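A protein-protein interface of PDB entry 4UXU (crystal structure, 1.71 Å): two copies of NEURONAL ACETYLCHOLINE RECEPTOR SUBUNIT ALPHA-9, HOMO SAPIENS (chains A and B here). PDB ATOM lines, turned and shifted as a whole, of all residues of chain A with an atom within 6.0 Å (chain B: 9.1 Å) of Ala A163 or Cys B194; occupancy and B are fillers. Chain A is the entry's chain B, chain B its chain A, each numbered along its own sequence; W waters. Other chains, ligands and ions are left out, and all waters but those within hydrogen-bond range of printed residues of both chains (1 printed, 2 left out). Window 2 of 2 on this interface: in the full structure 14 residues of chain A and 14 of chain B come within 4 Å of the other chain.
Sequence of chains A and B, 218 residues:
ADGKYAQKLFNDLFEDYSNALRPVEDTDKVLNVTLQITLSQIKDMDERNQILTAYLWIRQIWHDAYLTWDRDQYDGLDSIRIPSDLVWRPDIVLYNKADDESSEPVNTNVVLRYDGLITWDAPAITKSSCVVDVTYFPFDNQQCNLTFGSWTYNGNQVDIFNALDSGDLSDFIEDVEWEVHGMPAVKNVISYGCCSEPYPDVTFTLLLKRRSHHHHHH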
ATOM      1  N   THR A  34      10.088  -6.008   9.659  1.00  0.00           N
ATOM      2  CA  THR A  34      10.827  -7.090   9.037  1.00  0.00           C
ATOM      3  C   THR A  34      11.070  -6.749   7.579  1.00  0.00           C
ATOM      4  O   THR A  34      10.274  -6.055   6.945  1.00  0.00           O
ATOM      5  CB  THR A  34      10.113  -8.454   9.160  1.00  0.00           C
ATOM      6  OG1 THR A  34       8.896  -8.449   8.405  1.00  0.00           O
ATOM      7  CG2 THR A  34       9.818  -8.782  10.613  1.00  0.00           C
ATOM      8  N   LEU A  35      12.181  -7.236   7.054  1.00  0.00           N
ATOM      9  CA  LEU A  35      12.599  -6.905   5.702  1.00  0.00           C
ATOM     10  C   LEU A  35      12.854  -8.191   4.942  1.00  0.00           C
ATOM     11  O   LEU A  35      13.540  -9.071   5.442  1.00  0.00           O
ATOM     12  CB  LEU A  35      13.866  -6.048   5.727  1.00  0.00           C
ATOM     13  CG  LEU A  35      14.225  -5.158   4.531  1.00  0.00           C
ATOM     14  CD1 LEU A  35      15.419  -4.275   4.859  1.00  0.00           C
ATOM     15  CD2 LEU A  35      14.520  -5.964   3.291  1.00  0.00           C
ATOM     16  N   GLN A  36      12.292  -8.272   3.739  1.00  0.00           N
ATOM     17  CA  GLN A  36      12.549  -9.364   2.814  1.00  0.00           C
ATOM     18  C   GLN A  36      13.098  -8.780   1.519  1.00  0.00           C
ATOM     19  O   GLN A  36      12.538  -7.835   0.960  1.00  0.00           O
ATOM     20  CB  GLN A  36      11.278 -10.178   2.555  1.00  0.00           C
ATOM     21  CG  GLN A  36      11.397 -11.152   1.384  1.00  0.00           C
ATOM     22  CD  GLN A  36      10.271 -12.165   1.348  1.00  0.00           C
ATOM     23  OE1 GLN A  36       9.550 -12.349   2.330  1.00  0.00           O
ATOM     24  NE2 GLN A  36      10.133 -12.846   0.225  1.00  0.00           N
ATOM     25  N   ARG A  59      10.256  -6.165   0.458  1.00  0.00           N
ATOM     26  CA  ARG A  59       9.024  -6.275   1.235  1.00  0.00           C
ATOM     27  C   ARG A  59       9.279  -5.905   2.692  1.00  0.00           C
ATOM     28  O   ARG A  59      10.128  -6.508   3.372  1.00  0.00           O
ATOM     29  CB  ARG A  59       8.427  -7.687   1.152  1.00  0.00           C
ATOM     30  CG  ARG A  59       7.277  -7.917   2.126  1.00  0.00           C
ATOM     31  CD  ARG A  59       6.504  -9.215   1.835  1.00  0.00           C
ATOM     32  NE  ARG A  59       5.715  -9.111   0.595  1.00  0.00           N
ATOM     33  CZ  ARG A  59       4.725  -9.935   0.270  1.00  0.00           C
ATOM     34  NH1 ARG A  59       4.393 -10.929   1.088  1.00  0.00           N
ATOM     35  NH2 ARG A  59       4.063  -9.768  -0.877  1.00  0.00           N
ATOM     36  N   ILE A  61       7.369  -5.237   6.455  1.00  0.00           N
ATOM     37  CA  ILE A  61       6.199  -5.531   7.261  1.00  0.00           C
ATOM     38  C   ILE A  61       6.347  -4.934   8.653  1.00  0.00           C
ATOM     39  O   ILE A  61       7.368  -5.139   9.329  1.00  0.00           O
ATOM     40  CB  ILE A  61       5.960  -7.065   7.368  1.00  0.00           C
ATOM     41  CG1 ILE A  61       5.711  -7.651   5.981  1.00  0.00           C
ATOM     42  CG2 ILE A  61       4.788  -7.350   8.302  1.00  0.00           C
ATOM     43  CD1 ILE A  61       5.836  -9.162   5.915  1.00  0.00           C
ATOM     44  N   PHE A 161      14.514  -6.367  11.197  1.00  0.00           N
ATOM     45  CA  PHE A 161      14.770  -7.803  11.313  1.00  0.00           C
ATOM     46  C   PHE A 161      14.722  -8.440   9.945  1.00  0.00           C
ATOM     47  O   PHE A 161      13.979  -7.973   9.075  1.00  0.00           O
ATOM     48  CB  PHE A 161      13.735  -8.471  12.215  1.00  0.00           C
ATOM     49  CG  PHE A 161      13.714  -7.926  13.612  1.00  0.00           C
ATOM     50  CD1 PHE A 161      12.982  -6.788  13.906  1.00  0.00           C
ATOM     51  CD2 PHE A 161      14.424  -8.550  14.626  1.00  0.00           C
ATOM     52  CE1 PHE A 161      12.964  -6.266  15.181  1.00  0.00           C
ATOM     53  CE2 PHE A 161      14.413  -8.041  15.913  1.00  0.00           C
ATOM     54  CZ  PHE A 161      13.672  -6.890  16.188  1.00  0.00           C
ATOM     55  N   ASN A 162      15.523  -9.481   9.746  1.00  0.00           N
ATOM     56  CA  ASN A 162      15.423 -10.307   8.546  1.00  0.00           C
ATOM     57  C   ASN A 162      14.174 -11.157   8.592  1.00  0.00           C
ATOM     58  O   ASN A 162      13.951 -11.878   9.561  1.00  0.00           O
ATOM     59  CB  ASN A 162      16.657 -11.210   8.397  1.00  0.00           C
ATOM     60  CG  ASN A 162      17.824 -10.486   7.755  1.00  0.00           C
ATOM     61  OD1 ASN A 162      17.703  -9.963   6.654  1.00  0.00           O
ATOM     62  ND2 ASN A 162      18.946 -10.425   8.458  1.00  0.00           N
ATOM     63  N   ALA A 163      13.364 -11.093   7.545  1.00  0.00           N
ATOM     64  CA  ALA A 163      12.206 -11.967   7.473  1.00  0.00           C
ATOM     65  C   ALA A 163      12.636 -13.376   7.098  1.00  0.00           C
ATOM     66  O   ALA A 163      11.973 -14.340   7.455  1.00  0.00           O
ATOM     67  CB  ALA A 163      11.197 -11.444   6.475  1.00  0.00           C
ATOM     68  N   LEU A 164      13.742 -13.481   6.366  1.00  0.00           N
ATOM     69  CA  LEU A 164      14.220 -14.762   5.869  1.00  0.00           C
ATOM     70  C   LEU A 164      15.682 -15.012   6.226  1.00  0.00           C
ATOM     71  O   LEU A 164      16.381 -14.106   6.655  1.00  0.00           O
ATOM     72  CB  LEU A 164      14.045 -14.834   4.349  1.00  0.00           C
ATOM     73  CG  LEU A 164      12.603 -14.740   3.862  1.00  0.00           C
ATOM     74  CD1 LEU A 164      12.580 -14.841   2.349  1.00  0.00           C
ATOM     75  CD2 LEU A 164      11.750 -15.821   4.495  1.00  0.00           C
ATOM     76  N   ASP A 165      16.156 -16.240   6.027  1.00  0.00           N
ATOM     77  CA  ASP A 165      17.565 -16.542   6.284  1.00  0.00           C
ATOM     78  C   ASP A 165      18.472 -16.002   5.204  1.00  0.00           C
ATOM     79  O   ASP A 165      19.676 -15.836   5.409  1.00  0.00           O
ATOM     80  CB  ASP A 165      17.803 -18.060   6.388  1.00  0.00           C
ATOM     81  CG  ASP A 165      17.383 -18.632   7.720  1.00  0.00           C
ATOM     82  OD1 ASP A 165      17.197 -17.855   8.667  1.00  0.00           O
ATOM     83  OD2 ASP A 165      17.250 -19.875   7.824  1.00  0.00           O
ATOM     84  N   ALA A 185      21.682 -13.730   4.772  1.00  0.00           N
ATOM     85  CA  ALA A 185      21.341 -12.475   5.415  1.00  0.00           C
ATOM     86  C   ALA A 185      21.809 -12.464   6.865  1.00  0.00           C
ATOM     87  O   ALA A 185      21.679 -13.455   7.562  1.00  0.00           O
ATOM     88  CB  ALA A 185      19.846 -12.239   5.358  1.00  0.00           C
ATOM     89  N   SER B 191      23.386 -11.227  14.371  1.00  0.00           N
ATOM     90  CA  SER B 191      22.526 -12.394  14.377  1.00  0.00           C
ATOM     91  C   SER B 191      22.367 -12.859  12.946  1.00  0.00           C
ATOM     92  O   SER B 191      22.364 -12.052  12.013  1.00  0.00           O
ATOM     93  CB  SER B 191      21.176 -12.089  15.030  1.00  0.00           C
ATOM     94  OG  SER B 191      20.510 -11.024  14.391  1.00  0.00           O
ATOM     95  N   TYR B 192      22.257 -14.173  12.786  1.00  0.00           N
ATOM     96  CA  TYR B 192      22.226 -14.818  11.474  1.00  0.00           C
ATOM     97  C   TYR B 192      20.810 -15.203  11.053  1.00  0.00           C
ATOM     98  O   TYR B 192      20.055 -15.778  11.836  1.00  0.00           O
ATOM     99  CB  TYR B 192      23.126 -16.062  11.494  1.00  0.00           C
ATOM    100  CG  TYR B 192      24.585 -15.706  11.639  1.00  0.00           C
ATOM    101  CD1 TYR B 192      25.141 -15.463  12.887  1.00  0.00           C
ATOM    102  CD2 TYR B 192      25.397 -15.569  10.516  1.00  0.00           C
ATOM    103  CE1 TYR B 192      26.472 -15.108  13.018  1.00  0.00           C
ATOM    104  CE2 TYR B 192      26.723 -15.225  10.635  1.00  0.00           C
ATOM    105  CZ  TYR B 192      27.254 -14.990  11.887  1.00  0.00           C
ATOM    106  OH  TYR B 192      28.576 -14.644  12.008  1.00  0.00           O
ATOM    107  N   GLY B 193      20.449 -14.862   9.818  1.00  0.00           N
ATOM    108  CA  GLY B 193      19.153 -15.216   9.278  1.00  0.00           C
ATOM    109  C   GLY B 193      17.974 -14.641  10.047  1.00  0.00           C
ATOM    110  O   GLY B 193      18.085 -13.582  10.678  1.00  0.00           O
ATOM    111  N   CYS B 194      16.845 -15.342   9.976  1.00  0.00           N
ATOM    112  CA  CYS B 194      15.577 -14.868  10.524  1.00  0.00           C
ATOM    113  C   CYS B 194      15.549 -14.933  12.037  1.00  0.00           C
ATOM    114  O   CYS B 194      14.971 -14.072  12.697  1.00  0.00           O
ATOM    115  CB  CYS B 194      14.398 -15.696   9.979  1.00  0.00           C
ATOM    116  SG  CYS B 194      14.355 -17.396  10.582  1.00  0.00           S
ATOM    117  N   CYS B 195      16.162 -15.970  12.587  1.00  0.00           N
ATOM    118  CA  CYS B 195      15.730 -16.437  13.887  1.00  0.00           C
ATOM    119  C   CYS B 195      16.829 -16.824  14.875  1.00  0.00           C
ATOM    120  O   CYS B 195      16.528 -17.391  15.927  1.00  0.00           O
ATOM    121  CB  CYS B 195      14.797 -17.627  13.663  1.00  0.00           C
ATOM    122  SG  CYS B 195      13.461 -17.309  12.429  1.00  0.00           S
ATOM    123  N   SER B 196      18.088 -16.525  14.567  1.00  0.00           N
ATOM    124  CA  SER B 196      19.162 -16.953  15.462  1.00  0.00           C
ATOM    125  C   SER B 196      19.244 -16.069  16.708  1.00  0.00           C
ATOM    126  O   SER B 196      18.697 -14.971  16.758  1.00  0.00           O
ATOM    127  CB  SER B 196      20.523 -16.937  14.756  1.00  0.00           C
ATOM    128  OG  SER B 196      21.298 -15.799  15.162  1.00  0.00           O
ATOM    129  N   GLU B 197      19.926 -16.580  17.718  1.00  0.00           N
ATOM    130  CA  GLU B 197      20.271 -15.772  18.874  1.00  0.00           C
ATOM    131  C   GLU B 197      21.263 -14.670  18.486  1.00  0.00           C
ATOM    132  O   GLU B 197      21.945 -14.765  17.468  1.00  0.00           O
ATOM    133  CB  GLU B 197      20.846 -16.669  19.970  1.00  0.00           C
ATOM    134  CG  GLU B 197      19.841 -17.677  20.530  1.00  0.00           C
ATOM    135  CD  GLU B 197      18.618 -17.006  21.151  1.00  0.00           C
ATOM    136  OE1 GLU B 197      18.768 -16.301  22.171  1.00  0.00           O
ATOM    137  OE2 GLU B 197      17.504 -17.176  20.611  1.00  0.00           O
HETATM  138  O   HOH W   1      17.950 -18.131  11.390  1.00  0.00           O
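Water W1 lies within hydrogen-bond range of the side-chain carboxylate of Asp A165 (2.8 Å), the backbone NH of Cys B195 (3.0 Å), the backbone carbonyl oxygen of Tyr B192 (3.2 Å) and the backbone NH of Cys B194 (3.3 Å).
No position is printed for both chains.
Of the 9 pairs that touch across the chains among the printed residues, none has its exchanged pair printed and touching as well.
Of chain A, only Asn A162, Ala A163, Leu A164 and Asp A165 come within 4 Å of Cys B194.
Printed residues of chain A within 4 Å of Tyr B192: Ala A185 (3.9997 Å).
Printed residues of chain B within 4 Å of Ala A185: Tyr B192 (3.9997 Å) and Gly B193 (2.9 Å).
Printed residues of chain B within 4 Å of Asn A162: Gly B193 (3.6 Å) and Cys B194 (3.5 Å).
Thr A34 touches none of the printed residues of chain B.
The nearest residue of chain B that does not touch Ala A163 is Cys B195 (6.0 Å).
The nearest residue of chain A that does not touch Cys B194 is Ala A185 (5.7 Å).
Of the 7 printed residues of chain B, 3 touch a printed residue of chain A.
Printed residues of chain B that touch a printed residue of chain A: Tyr B192, Gly B193 and Cys B194.
Of the 11 printed residues of chain A, 5 touch a printed residue of chain B.
Among the printed residues, 9 pairs touch across the chains.
The backbone carbonyl oxygen (O) of Ala A185 lies within hydrogen-bond range of the backbone NH (N) of Gly B193.
The backbone NH (N) of Cys B194 lies within hydrogen-bond range of the side-chain carboxylate (OD1) of Asp A165.
The backbone NH (N) of Tyr B192 sits at hydrogen-bond distance from the side-chain hydroxyl (OG) of Ser B196 (3.0 Å).
SG of Cys B194 is disulfide-bonded to SG of Cys B195, 2.1 Å away.
The backbone NH of Ala A163 is in hydrogen-bond range of the backbone carbonyl oxygen of Leu A35 (2.9 Å).
The backbone carbonyl oxygen (O) of Asp A165 sits at hydrogen-bond distance from the backbone NH (N) of Ala A185, at 3.0 Å.
Among the printed residues, pairs that only touch across the chains: Asp A165 with Gly B193, Asn A162 with Cys B194, Leu A164 with Cys B194, Asn A162 with Gly B193, Ala A163 with Cys B194, Leu A164 with Gly B193 and Ala A185 with Tyr B192.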
